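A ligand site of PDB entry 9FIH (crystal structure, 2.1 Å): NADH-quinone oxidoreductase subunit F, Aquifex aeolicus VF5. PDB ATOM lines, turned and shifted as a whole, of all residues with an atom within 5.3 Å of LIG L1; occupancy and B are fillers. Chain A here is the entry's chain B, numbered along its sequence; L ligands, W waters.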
ATOM      1  N   GLY A  67      14.409  -4.132  -8.010  1.00  0.00           N
ATOM      2  CA  GLY A  67      15.751  -4.522  -8.415  1.00  0.00           C
ATOM      3  C   GLY A  67      16.362  -3.470  -9.329  1.00  0.00           C
ATOM      4  O   GLY A  67      17.563  -3.494  -9.567  1.00  0.00           O
ATOM      5  N   GLY A  68      15.531  -2.567  -9.868  1.00  0.00           N
ATOM      6  CA  GLY A  68      16.030  -1.478 -10.690  1.00  0.00           C
ATOM      7  C   GLY A  68      15.282  -1.328 -12.007  1.00  0.00           C
ATOM      8  O   GLY A  68      15.247  -0.225 -12.536  1.00  0.00           O
ATOM      9  N   ALA A  69      14.693  -2.407 -12.558  1.00  0.00           N
ATOM     10  CA  ALA A  69      14.007  -2.296 -13.842  1.00  0.00           C
ATOM     11  C   ALA A  69      12.537  -1.889 -13.693  1.00  0.00           C
ATOM     12  O   ALA A  69      11.925  -1.418 -14.647  1.00  0.00           O
ATOM     13  CB  ALA A  69      14.126  -3.575 -14.632  1.00  0.00           C
ATOM     14  N   PHE A  71       9.770  -3.724 -13.323  1.00  0.00           N
ATOM     15  CA  PHE A  71       8.750  -4.520 -14.004  1.00  0.00           C
ATOM     16  C   PHE A  71       7.586  -4.842 -13.046  1.00  0.00           C
ATOM     17  O   PHE A  71       7.840  -5.233 -11.906  1.00  0.00           O
ATOM     18  CB  PHE A  71       9.360  -5.811 -14.536  1.00  0.00           C
ATOM     19  CG  PHE A  71       8.409  -6.501 -15.490  1.00  0.00           C
ATOM     20  CD1 PHE A  71       8.409  -6.197 -16.851  1.00  0.00           C
ATOM     21  CD2 PHE A  71       7.466  -7.418 -15.021  1.00  0.00           C
ATOM     22  CE1 PHE A  71       7.522  -6.808 -17.723  1.00  0.00           C
ATOM     23  CE2 PHE A  71       6.591  -8.035 -15.896  1.00  0.00           C
ATOM     24  CZ  PHE A  71       6.615  -7.723 -17.244  1.00  0.00           C
ATOM     25  N   LYS A  76       4.342 -10.353 -13.590  1.00  0.00           N
ATOM     26  CA  LYS A  76       5.415 -11.345 -13.668  1.00  0.00           C
ATOM     27  C   LYS A  76       4.920 -12.685 -13.127  1.00  0.00           C
ATOM     28  O   LYS A  76       5.160 -13.734 -13.734  1.00  0.00           O
ATOM     29  CB  LYS A  76       6.678 -10.891 -12.922  1.00  0.00           C
ATOM     30  CG  LYS A  76       7.876 -11.787 -13.107  1.00  0.00           C
ATOM     31  CD  LYS A  76       9.109 -11.395 -12.297  1.00  0.00           C
ATOM     32  CE  LYS A  76       9.616  -9.993 -12.524  1.00  0.00           C
ATOM     33  NZ  LYS A  76      10.897  -9.816 -11.846  1.00  0.00           N
ATOM     34  N   PHE A  79       2.386 -14.416 -15.356  1.00  0.00           N
ATOM     35  CA  PHE A  79       3.061 -15.055 -16.486  1.00  0.00           C
ATOM     36  C   PHE A  79       3.575 -16.437 -16.105  1.00  0.00           C
ATOM     37  O   PHE A  79       3.385 -17.399 -16.853  1.00  0.00           O
ATOM     38  CB  PHE A  79       4.209 -14.176 -17.003  1.00  0.00           C
ATOM     39  CG  PHE A  79       3.810 -12.973 -17.848  1.00  0.00           C
ATOM     40  CD1 PHE A  79       2.727 -13.014 -18.717  1.00  0.00           C
ATOM     41  CD2 PHE A  79       4.558 -11.803 -17.808  1.00  0.00           C
ATOM     42  CE1 PHE A  79       2.401 -11.918 -19.510  1.00  0.00           C
ATOM     43  CE2 PHE A  79       4.232 -10.718 -18.611  1.00  0.00           C
ATOM     44  CZ  PHE A  79       3.151 -10.766 -19.430  1.00  0.00           C
ATOM     45  N   ASP A  94      21.789 -10.373  -4.630  1.00  0.00           N
ATOM     46  CA  ASP A  94      23.158 -10.223  -5.118  1.00  0.00           C
ATOM     47  C   ASP A  94      23.673  -8.796  -4.922  1.00  0.00           C
ATOM     48  O   ASP A  94      24.883  -8.620  -4.908  1.00  0.00           O
ATOM     49  CB  ASP A  94      23.328 -10.672  -6.558  1.00  0.00           C
ATOM     50  CG  ASP A  94      24.767 -10.935  -6.940  1.00  0.00           C
ATOM     51  OD1 ASP A  94      25.362 -11.863  -6.348  1.00  0.00           O
ATOM     52  OD2 ASP A  94      25.298 -10.183  -7.787  1.00  0.00           O
ATOM     53  N   GLU A  95      22.761  -7.815  -4.747  1.00  0.00           N
ATOM     54  CA  GLU A  95      23.038  -6.393  -4.632  1.00  0.00           C
ATOM     55  C   GLU A  95      24.520  -6.039  -4.737  1.00  0.00           C
ATOM     56  O   GLU A  95      25.227  -6.040  -3.731  1.00  0.00           O
ATOM     57  CB  GLU A  95      22.471  -5.892  -3.294  1.00  0.00           C
ATOM     58  CG  GLU A  95      22.696  -4.408  -3.010  1.00  0.00           C
ATOM     59  CD  GLU A  95      21.910  -3.880  -1.808  1.00  0.00           C
ATOM     60  OE1 GLU A  95      22.265  -4.216  -0.642  1.00  0.00           O
ATOM     61  OE2 GLU A  95      20.944  -3.126  -2.082  1.00  0.00           O
ATOM     62  N   SER A  96      24.971  -5.674  -5.949  1.00  0.00           N
ATOM     63  CA  SER A  96      26.367  -5.321  -6.188  1.00  0.00           C
ATOM     64  C   SER A  96      26.564  -4.060  -7.032  1.00  0.00           C
ATOM     65  O   SER A  96      27.693  -3.749  -7.385  1.00  0.00           O
ATOM     66  CB  SER A  96      27.075  -6.462  -6.853  1.00  0.00           C
ATOM     67  OG  SER A  96      27.246  -7.554  -5.976  1.00  0.00           O
ATOM     68  N   GLU A  97      25.471  -3.355  -7.349  1.00  0.00           N
ATOM     69  CA  GLU A  97      25.548  -2.072  -8.044  1.00  0.00           C
ATOM     70  C   GLU A  97      26.305  -1.065  -7.169  1.00  0.00           C
ATOM     71  O   GLU A  97      25.994  -0.938  -5.988  1.00  0.00           O
ATOM     72  CB  GLU A  97      24.151  -1.535  -8.345  1.00  0.00           C
ATOM     73  CG  GLU A  97      24.126  -0.238  -9.139  1.00  0.00           C
ATOM     74  CD  GLU A  97      24.335  -0.376 -10.637  1.00  0.00           C
ATOM     75  OE1 GLU A  97      24.741  -1.472 -11.090  1.00  0.00           O
ATOM     76  OE2 GLU A  97      24.085   0.631 -11.346  1.00  0.00           O
ATOM     77  N   THR A 100      24.915   0.940  -3.901  1.00  0.00           N
ATOM     78  CA  THR A 100      23.651   0.286  -3.600  1.00  0.00           C
ATOM     79  C   THR A 100      23.808  -0.652  -2.382  1.00  0.00           C
ATOM     80  O   THR A 100      24.542  -1.643  -2.436  1.00  0.00           O
ATOM     81  CB  THR A 100      23.103  -0.439  -4.838  1.00  0.00           C
ATOM     82  OG1 THR A 100      23.091   0.522  -5.903  1.00  0.00           O
ATOM     83  CG2 THR A 100      21.697  -0.971  -4.595  1.00  0.00           C
ATOM     84  N   LYS A 102      20.754  -0.955  -0.028  1.00  0.00           N
ATOM     85  CA  LYS A 102      19.401  -0.914   0.517  1.00  0.00           C
ATOM     86  C   LYS A 102      18.955  -2.312   0.956  1.00  0.00           C
ATOM     87  O   LYS A 102      18.326  -2.463   2.011  1.00  0.00           O
ATOM     88  CB  LYS A 102      18.505  -0.289  -0.563  1.00  0.00           C
ATOM     89  CG  LYS A 102      18.425  -1.092  -1.863  1.00  0.00           C
ATOM     90  CD  LYS A 102      17.551  -0.446  -2.934  1.00  0.00           C
ATOM     91  CE  LYS A 102      17.346  -1.347  -4.113  1.00  0.00           C
ATOM     92  NZ  LYS A 102      16.539  -2.527  -3.786  1.00  0.00           N
ATOM     93  N   ASP A 103      19.277  -3.349   0.184  1.00  0.00           N
ATOM     94  CA  ASP A 103      18.728  -4.664   0.453  1.00  0.00           C
ATOM     95  C   ASP A 103      19.371  -5.264   1.696  1.00  0.00           C
ATOM     96  O   ASP A 103      18.679  -5.939   2.469  1.00  0.00           O
ATOM     97  CB  ASP A 103      18.897  -5.626  -0.717  1.00  0.00           C
ATOM     98  CG  ASP A 103      18.239  -5.216  -2.017  1.00  0.00           C
ATOM     99  OD1 ASP A 103      17.357  -4.334  -1.995  1.00  0.00           O
ATOM    100  OD2 ASP A 103      18.651  -5.788  -3.068  1.00  0.00           O
ATOM    101  N   TYR A 180      29.495  -9.525 -10.142  1.00  0.00           N
ATOM    102  CA  TYR A 180      28.347  -8.634 -10.267  1.00  0.00           C
ATOM    103  C   TYR A 180      27.309  -9.206 -11.223  1.00  0.00           C
ATOM    104  O   TYR A 180      26.114  -9.006 -11.026  1.00  0.00           O
ATOM    105  CB  TYR A 180      28.901  -7.300 -10.760  1.00  0.00           C
ATOM    106  CG  TYR A 180      27.935  -6.290 -11.363  1.00  0.00           C
ATOM    107  CD1 TYR A 180      27.122  -5.502 -10.566  1.00  0.00           C
ATOM    108  CD2 TYR A 180      27.873  -6.088 -12.732  1.00  0.00           C
ATOM    109  CE1 TYR A 180      26.267  -4.572 -11.125  1.00  0.00           C
ATOM    110  CE2 TYR A 180      27.027  -5.150 -13.297  1.00  0.00           C
ATOM    111  CZ  TYR A 180      26.221  -4.367 -12.495  1.00  0.00           C
ATOM    112  OH  TYR A 180      25.397  -3.424 -13.026  1.00  0.00           O
ATOM    113  N   GLU A 184      22.334 -10.522 -12.502  1.00  0.00           N
ATOM    114  CA  GLU A 184      21.471 -10.640 -13.673  1.00  0.00           C
ATOM    115  C   GLU A 184      20.733 -11.981 -13.535  1.00  0.00           C
ATOM    116  O   GLU A 184      21.357 -13.022 -13.304  1.00  0.00           O
ATOM    117  CB  GLU A 184      22.310 -10.507 -14.942  1.00  0.00           C
ATOM    118  CG  GLU A 184      21.496 -10.191 -16.187  1.00  0.00           C
ATOM    119  CD  GLU A 184      20.831 -11.384 -16.856  1.00  0.00           C
ATOM    120  OE1 GLU A 184      21.132 -12.518 -16.494  1.00  0.00           O
ATOM    121  OE2 GLU A 184      19.999 -11.144 -17.757  1.00  0.00           O
ATOM    122  N   GLU A 185      19.391 -11.931 -13.644  1.00  0.00           N
ATOM    123  CA  GLU A 185      18.562 -13.058 -13.198  1.00  0.00           C
ATOM    124  C   GLU A 185      18.941 -14.381 -13.884  1.00  0.00           C
ATOM    125  O   GLU A 185      18.863 -15.434 -13.267  1.00  0.00           O
ATOM    126  CB  GLU A 185      17.094 -12.718 -13.388  1.00  0.00           C
ATOM    127  CG  GLU A 185      16.703 -12.414 -14.828  1.00  0.00           C
ATOM    128  CD  GLU A 185      15.226 -12.121 -15.049  1.00  0.00           C
ATOM    129  OE1 GLU A 185      14.468 -12.156 -14.057  1.00  0.00           O
ATOM    130  OE2 GLU A 185      14.851 -11.856 -16.214  1.00  0.00           O
ATOM    131  N   TYR A 205      12.095 -15.458 -20.971  1.00  0.00           N
ATOM    132  CA  TYR A 205      12.240 -14.917 -19.632  1.00  0.00           C
ATOM    133  C   TYR A 205      12.147 -16.083 -18.650  1.00  0.00           C
ATOM    134  O   TYR A 205      11.543 -17.097 -18.963  1.00  0.00           O
ATOM    135  CB  TYR A 205      11.179 -13.841 -19.375  1.00  0.00           C
ATOM    136  CG  TYR A 205      11.377 -12.621 -20.258  1.00  0.00           C
ATOM    137  CD1 TYR A 205      12.303 -11.638 -19.937  1.00  0.00           C
ATOM    138  CD2 TYR A 205      10.623 -12.456 -21.417  1.00  0.00           C
ATOM    139  CE1 TYR A 205      12.507 -10.543 -20.770  1.00  0.00           C
ATOM    140  CE2 TYR A 205      10.798 -11.357 -22.244  1.00  0.00           C
ATOM    141  CZ  TYR A 205      11.748 -10.412 -21.913  1.00  0.00           C
ATOM    142  OH  TYR A 205      11.934  -9.325 -22.708  1.00  0.00           O
ATOM    143  N   PRO A 206      12.738 -15.957 -17.442  1.00  0.00           N
ATOM    144  CA  PRO A 206      12.715 -17.036 -16.458  1.00  0.00           C
ATOM    145  C   PRO A 206      11.337 -17.628 -16.153  1.00  0.00           C
ATOM    146  O   PRO A 206      11.233 -18.824 -15.948  1.00  0.00           O
ATOM    147  CB  PRO A 206      13.364 -16.379 -15.229  1.00  0.00           C
ATOM    148  CG  PRO A 206      14.298 -15.346 -15.831  1.00  0.00           C
ATOM    149  CD  PRO A 206      13.474 -14.776 -16.964  1.00  0.00           C
ATOM    150  N   VAL A 207      10.291 -16.786 -16.173  1.00  0.00           N
ATOM    151  CA  VAL A 207       8.925 -17.221 -15.878  1.00  0.00           C
ATOM    152  C   VAL A 207       8.462 -18.268 -16.889  1.00  0.00           C
ATOM    153  O   VAL A 207       7.516 -19.029 -16.604  1.00  0.00           O
ATOM    154  CB  VAL A 207       7.892 -16.078 -15.793  1.00  0.00           C
ATOM    155  CG1 VAL A 207       8.177 -15.163 -14.616  1.00  0.00           C
ATOM    156  CG2 VAL A 207       7.792 -15.288 -17.091  1.00  0.00           C
ATOM    157  N   VAL A 218      12.070 -14.615 -10.461  1.00  0.00           N
ATOM    158  CA  VAL A 218      13.148 -13.958  -9.755  1.00  0.00           C
ATOM    159  C   VAL A 218      12.632 -12.590  -9.323  1.00  0.00           C
ATOM    160  O   VAL A 218      12.195 -11.784 -10.153  1.00  0.00           O
ATOM    161  CB  VAL A 218      14.437 -13.829 -10.580  1.00  0.00           C
ATOM    162  CG1 VAL A 218      15.576 -13.197  -9.787  1.00  0.00           C
ATOM    163  CG2 VAL A 218      14.901 -15.159 -11.157  1.00  0.00           C
ATOM    164  N   ASN A 220      13.655  -9.174  -6.520  1.00  0.00           N
ATOM    165  CA  ASN A 220      14.601  -8.490  -5.663  1.00  0.00           C
ATOM    166  C   ASN A 220      14.134  -8.502  -4.196  1.00  0.00           C
ATOM    167  O   ASN A 220      12.932  -8.503  -3.942  1.00  0.00           O
ATOM    168  CB  ASN A 220      14.839  -7.086  -6.215  1.00  0.00           C
ATOM    169  CG  ASN A 220      15.694  -6.254  -5.308  1.00  0.00           C
ATOM    170  OD1 ASN A 220      16.930  -6.433  -5.250  1.00  0.00           O
ATOM    171  ND2 ASN A 220      15.057  -5.333  -4.595  1.00  0.00           N
ATOM    172  N   LEU A 297      24.479   3.477 -13.575  1.00  0.00           N
ATOM    173  CA  LEU A 297      23.517   3.460 -14.670  1.00  0.00           C
ATOM    174  C   LEU A 297      23.352   4.839 -15.326  1.00  0.00           C
ATOM    175  O   LEU A 297      23.349   4.941 -16.558  1.00  0.00           O
ATOM    176  CB  LEU A 297      22.202   2.925 -14.127  1.00  0.00           C
ATOM    177  CG  LEU A 297      21.052   2.746 -15.127  1.00  0.00           C
ATOM    178  CD1 LEU A 297      21.394   1.702 -16.168  1.00  0.00           C
ATOM    179  CD2 LEU A 297      19.757   2.382 -14.415  1.00  0.00           C
ATOM    180  N   GLY A 318      15.654   3.371 -11.754  1.00  0.00           N
ATOM    181  CA  GLY A 318      16.774   2.600 -11.244  1.00  0.00           C
ATOM    182  C   GLY A 318      16.468   1.938  -9.904  1.00  0.00           C
ATOM    183  O   GLY A 318      15.329   1.598  -9.622  1.00  0.00           O
ATOM    184  N   THR A 319      17.523   1.749  -9.093  1.00  0.00           N
ATOM    185  CA  THR A 319      17.418   1.205  -7.749  1.00  0.00           C
ATOM    186  C   THR A 319      17.054   2.288  -6.740  1.00  0.00           C
ATOM    187  O   THR A 319      16.874   1.963  -5.575  1.00  0.00           O
ATOM    188  CB  THR A 319      18.753   0.563  -7.359  1.00  0.00           C
ATOM    189  OG1 THR A 319      19.736   1.587  -7.530  1.00  0.00           O
ATOM    190  CG2 THR A 319      19.153  -0.592  -8.252  1.00  0.00           C
ATOM    191  N   GLY A 394      21.885  -6.752 -19.834  1.00  0.00           N
ATOM    192  CA  GLY A 394      21.765  -5.324 -19.590  1.00  0.00           C
ATOM    193  C   GLY A 394      23.114  -4.675 -19.311  1.00  0.00           C
ATOM    194  O   GLY A 394      23.238  -3.457 -19.426  1.00  0.00           O
HETATM  195  P1  LIG L   1      14.449  -6.087 -17.697  1.00  0.00           P
HETATM  196  O1  LIG L   1      13.793  -4.789 -17.900  1.00  0.00           O
HETATM  197  O2  LIG L   1      14.910  -6.768 -18.900  1.00  0.00           O
HETATM  198  O3  LIG L   1      13.523  -7.171 -16.940  1.00  0.00           O
HETATM  199  C1  LIG L   1      12.972  -6.848 -15.632  1.00  0.00           C
HETATM  200  C2  LIG L   1      12.281  -8.028 -15.037  1.00  0.00           C
HETATM  201  O4  LIG L   1      11.031  -8.207 -15.743  1.00  0.00           O
HETATM  202  C3  LIG L   1      13.023  -9.350 -15.155  1.00  0.00           C
HETATM  203  O5  LIG L   1      12.732 -10.204 -14.054  1.00  0.00           O
HETATM  204  C4  LIG L   1      12.463  -9.943 -16.448  1.00  0.00           C
HETATM  205  O6  LIG L   1      12.484 -11.356 -16.424  1.00  0.00           O
HETATM  206  C5  LIG L   1      11.009  -9.465 -16.373  1.00  0.00           C
HETATM  207  N1  LIG L   1      10.372  -9.288 -17.664  1.00  0.00           N
HETATM  208  C6  LIG L   1      10.579  -8.268 -18.552  1.00  0.00           C
HETATM  209  N2  LIG L   1       9.867  -8.344 -19.641  1.00  0.00           N
HETATM  210  C7  LIG L   1       9.126  -9.504 -19.467  1.00  0.00           C
HETATM  211  C8  LIG L   1       8.184 -10.139 -20.284  1.00  0.00           C
HETATM  212  N3  LIG L   1       7.810  -9.685 -21.471  1.00  0.00           N
HETATM  213  N4  LIG L   1       7.624 -11.281 -19.818  1.00  0.00           N
HETATM  214  C9  LIG L   1       8.001 -11.737 -18.618  1.00  0.00           C
HETATM  215  N5  LIG L   1       8.888 -11.228 -17.763  1.00  0.00           N
HETATM  216  C10 LIG L   1       9.429 -10.095 -18.250  1.00  0.00           C
HETATM  217  O7  LIG L   1      15.723  -5.788 -16.798  1.00  0.00           O
HETATM  218  P2  LIG L   1      16.979  -6.591 -16.272  1.00  0.00           P
HETATM  219  O8  LIG L   1      17.888  -6.735 -17.485  1.00  0.00           O
HETATM  220  O9  LIG L   1      16.665  -7.918 -15.639  1.00  0.00           O
HETATM  221  O10 LIG L   1      17.642  -5.618 -15.200  1.00  0.00           O
HETATM  222  C11 LIG L   1      18.214  -4.312 -15.489  1.00  0.00           C
HETATM  223  C12 LIG L   1      18.263  -3.513 -14.207  1.00  0.00           C
HETATM  224  O11 LIG L   1      19.169  -4.133 -13.275  1.00  0.00           O
HETATM  225  C13 LIG L   1      18.788  -2.076 -14.348  1.00  0.00           C
HETATM  226  O12 LIG L   1      17.716  -1.152 -14.434  1.00  0.00           O
HETATM  227  C14 LIG L   1      19.570  -1.841 -13.034  1.00  0.00           C
HETATM  228  O13 LIG L   1      18.998  -0.790 -12.271  1.00  0.00           O
HETATM  229  C15 LIG L   1      19.387  -3.155 -12.278  1.00  0.00           C
HETATM  230  N6  LIG L   1      20.556  -3.555 -11.490  1.00  0.00           N
HETATM  231  C16 LIG L   1      20.495  -3.701 -10.111  1.00  0.00           C
HETATM  232  C17 LIG L   1      21.573  -4.032  -9.366  1.00  0.00           C
HETATM  233  C18 LIG L   1      21.448  -4.116  -7.860  1.00  0.00           C
HETATM  234  O14 LIG L   1      22.460  -4.375  -7.190  1.00  0.00           O
HETATM  235  N7  LIG L   1      20.241  -3.937  -7.313  1.00  0.00           N
HETATM  236  C19 LIG L   1      22.898  -4.318 -10.023  1.00  0.00           C
HETATM  237  C20 LIG L   1      22.837  -4.127 -11.482  1.00  0.00           C
HETATM  238  C21 LIG L   1      21.746  -3.769 -12.123  1.00  0.00           C
HETATM  239  C1  LG2 L   2      20.636  -7.071 -12.469  1.00  0.00           C
HETATM  240  N1  LG2 L   2      19.476  -7.146 -11.636  1.00  0.00           N
HETATM  241  C2  LG2 L   2      19.631  -7.285 -10.260  1.00  0.00           C
HETATM  242  N2  LG2 L   2      18.503  -7.383  -9.474  1.00  0.00           N
HETATM  243  C3  LG2 L   2      18.568  -7.573  -8.119  1.00  0.00           C
HETATM  244  O1  LG2 L   2      17.581  -7.813  -7.447  1.00  0.00           O
HETATM  245  N3  LG2 L   2      19.820  -7.547  -7.559  1.00  0.00           N
HETATM  246  C4  LG2 L   2      21.016  -7.468  -8.242  1.00  0.00           C
HETATM  247  O2  LG2 L   2      22.063  -7.510  -7.615  1.00  0.00           O
HETATM  248  C5  LG2 L   2      20.863  -7.344  -9.673  1.00  0.00           C
HETATM  249  N4  LG2 L   2      21.978  -7.296 -10.469  1.00  0.00           N
HETATM  250  C6  LG2 L   2      21.889  -7.170 -11.850  1.00  0.00           C
HETATM  251  C7  LG2 L   2      23.041  -7.120 -12.636  1.00  0.00           C
HETATM  252  C8  LG2 L   2      22.971  -6.949 -14.003  1.00  0.00           C
HETATM  253  C9  LG2 L   2      24.238  -6.912 -14.825  1.00  0.00           C
HETATM  254  C10 LG2 L   2      21.721  -6.828 -14.624  1.00  0.00           C
HETATM  255  C11 LG2 L   2      21.641  -6.509 -16.094  1.00  0.00           C
HETATM  256  C12 LG2 L   2      20.569  -6.898 -13.857  1.00  0.00           C
HETATM  257  C13 LG2 L   2      18.120  -7.122 -12.219  1.00  0.00           C
HETATM  258  C14 LG2 L   2      17.656  -8.568 -12.405  1.00  0.00           C
HETATM  259  O3  LG2 L   2      18.125  -9.096 -13.653  1.00  0.00           O
HETATM  260  C15 LG2 L   2      16.121  -8.631 -12.348  1.00  0.00           C
HETATM  261  O4  LG2 L   2      15.601  -7.566 -13.133  1.00  0.00           O
HETATM  262  C16 LG2 L   2      15.517  -8.522 -10.950  1.00  0.00           C
HETATM  263  O5  LG2 L   2      16.188  -9.329  -9.981  1.00  0.00           O
HETATM  264  C17 LG2 L   2      14.049  -8.862 -10.991  1.00  0.00           C
HETATM  265  O6  LG2 L   2      13.431  -8.589  -9.713  1.00  0.00           O
HETATM  266  P1  LG2 L   2      12.410  -7.339  -9.546  1.00  0.00           P
HETATM  267  O7  LG2 L   2      11.837  -7.583  -8.147  1.00  0.00           O
HETATM  268  O8  LG2 L   2      11.363  -7.449 -10.628  1.00  0.00           O
HETATM  269  O9  LG2 L   2      13.212  -6.056  -9.613  1.00  0.00           O
HETATM  270  O   HOH W   1      11.909 -13.420 -13.410  1.00  0.00           O
HETATM  271  O   HOH W   2      19.679  -3.583  -4.452  1.00  0.00           O
HETATM  272  O   HOH W   3      11.228  -4.556 -18.295  1.00  0.00           O
HETATM  273  O   HOH W   4      22.827  -2.471 -15.074  1.00  0.00           O
HETATM  274  O   HOH W   5      10.501 -12.994 -15.815  1.00  0.00           O
HETATM  275  O   HOH W   6      21.314   0.753 -11.067  1.00  0.00           O
HETATM  276  O   HOH W   7      16.691 -10.155 -17.484  1.00  0.00           O
HETATM  277  O   HOH W   8      18.000  -4.625 -19.299  1.00  0.00           O
HETATM  278  O   HOH W   9      19.539  -8.471 -18.636  1.00  0.00           O
HETATM  279  O   HOH W  10       5.806 -12.510 -21.586  1.00  0.00           O
HETATM  280  O   HOH W  11      15.286  -2.281 -17.853  1.00  0.00           O
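The backbone NH (N) of Gly 67 lies within hydrogen-bond range of an oxygen (O9) of LG2 L2, 2.8 Å away. N of Glu 95 lies within hydrogen-bond range of O2 of LG2 L2 (3.0 Å). The backbone NH (N) of Asn 220 sits at hydrogen-bond distance from an oxygen (O7) of LG2 L2 (2.9 Å). An oxygen (O6) of LIG L1 sits at hydrogen-bond distance from the side-chain carboxylate of Glu 185. An oxygen (O14) of LIG L1 lies within hydrogen-bond range of the backbone NH (N) of Ser 96. The backbone NH of Glu 185 sits at hydrogen-bond distance from an oxygen (O3) of LG2 L2 (3.1 Å). The side-chain amino group (NZ) of Lys 76 lies within salt-bridge range of an oxygen (O8) of LG2 L2 (2.7 Å). An oxygen (O12) of LIG L1 lies within hydrogen-bond range of the backbone carbonyl oxygen of Gly 68, at 3.2 Å. OD1 of Asn 220 sits close to O1 of LG2 L2 (2.7 Å). N of Glu 97 lies within hydrogen-bond range of O14 of LIG L1, 3.2 Å away. O5 of LIG L1 sits at hydrogen-bond distance from NZ of Lys 76 (2.9 Å).
An oxygen (O3) of LG2 L2 sits at hydrogen-bond distance from an oxygen (O9) of LIG L1 (2.7 Å).
The side-chain hydroxyl (OG) of Ser 96 is in hydrogen-bond range of the backbone carbonyl oxygen (O) of Asp 94 (2.8 Å). The backbone NH (N) of Lys 102 sits at hydrogen-bond distance from the side-chain carboxylate (OE2) of Glu 95, at 3.0 Å. The side-chain amino group (NZ) of Lys 76 sits at hydrogen-bond distance from the backbone carbonyl oxygen (O) of Val 218 (2.9 Å). The backbone carbonyl oxygen (O) of Glu 97 lies close to the side-chain hydroxyl (OG1) of Thr 100 (3.3 Å). OE2 of Glu 95 lies within hydrogen-bond range of N of Asp 103 (2.8 Å). The side-chain hydroxyl of Tyr 180 sits at hydrogen-bond distance from the side-chain carboxylate of Glu 97 (2.8 Å).
Gly 67 touches LIG L1. Ala 69 touches LIG L1. Phe 71 touches LIG L1. CD2 of Phe 79 touches C9 of LIG L1, at 3.5 Å. Glu 95 touches LIG L1 (CA to O14, 3.3 Å). Tyr 180 touches LIG L1. Tyr 205 touches LIG L1 (CE2 to C8, 3.5 Å). Pro 206 touches LIG L1. Val 207 touches LIG L1. Leu 297 touches LIG L1. Thr 319 touches LIG L1 (CG2 to N7, 3.6 Å). Hydrophobic or aromatic side chains within 4 Å of LIG L1: Ala 69, Phe 71, Phe 79, Tyr 180, Tyr 205, Pro 206, Val 207 and Leu 297. 16 residues have an atom within 4 Å of LIG L1: Gly 67, Gly 68, Ala 69, Phe 71, Lys 76, Phe 79, Glu 95, Ser 96, Glu 97, Tyr 180, Glu 185, Tyr 205, Pro 206, Val 207, Leu 297 and Thr 319. The nearest printed residue that does not touch LIG L1 is Gly 318 (4.2 Å).
Water W9 lies within hydrogen-bond range of an oxygen (O8) of LIG L1 (2.7 Å), the side-chain carboxylate of Glu 184 (2.9 Å) and the backbone NH of Gly 394 (3.1 Å). Water W7 lies within hydrogen-bond range of OE2 of Glu 185 (2.8 Å), O9 of LIG L1 (2.9 Å) and OE2 of Glu 184 (3.5 Å). Water W2 lies within hydrogen-bond range of the side-chain carboxylate of Glu 95 (2.7 Å), the side-chain carboxylate of Asp 103 (2.8 Å), a nitrogen (N7) of LIG L1 (2.9 Å) and the side-chain amino group of Lys 102 (3.4 Å). Water W6 bridges OE2 of Glu 97 (2.8 Å) and O13 of LIG L1 (3.0 Å). Water W1 lies within hydrogen-bond range of OE1 of Glu 185 (2.9 Å), N of Val 218 (3.2 Å) and O5 of LIG L1 (3.4 Å).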
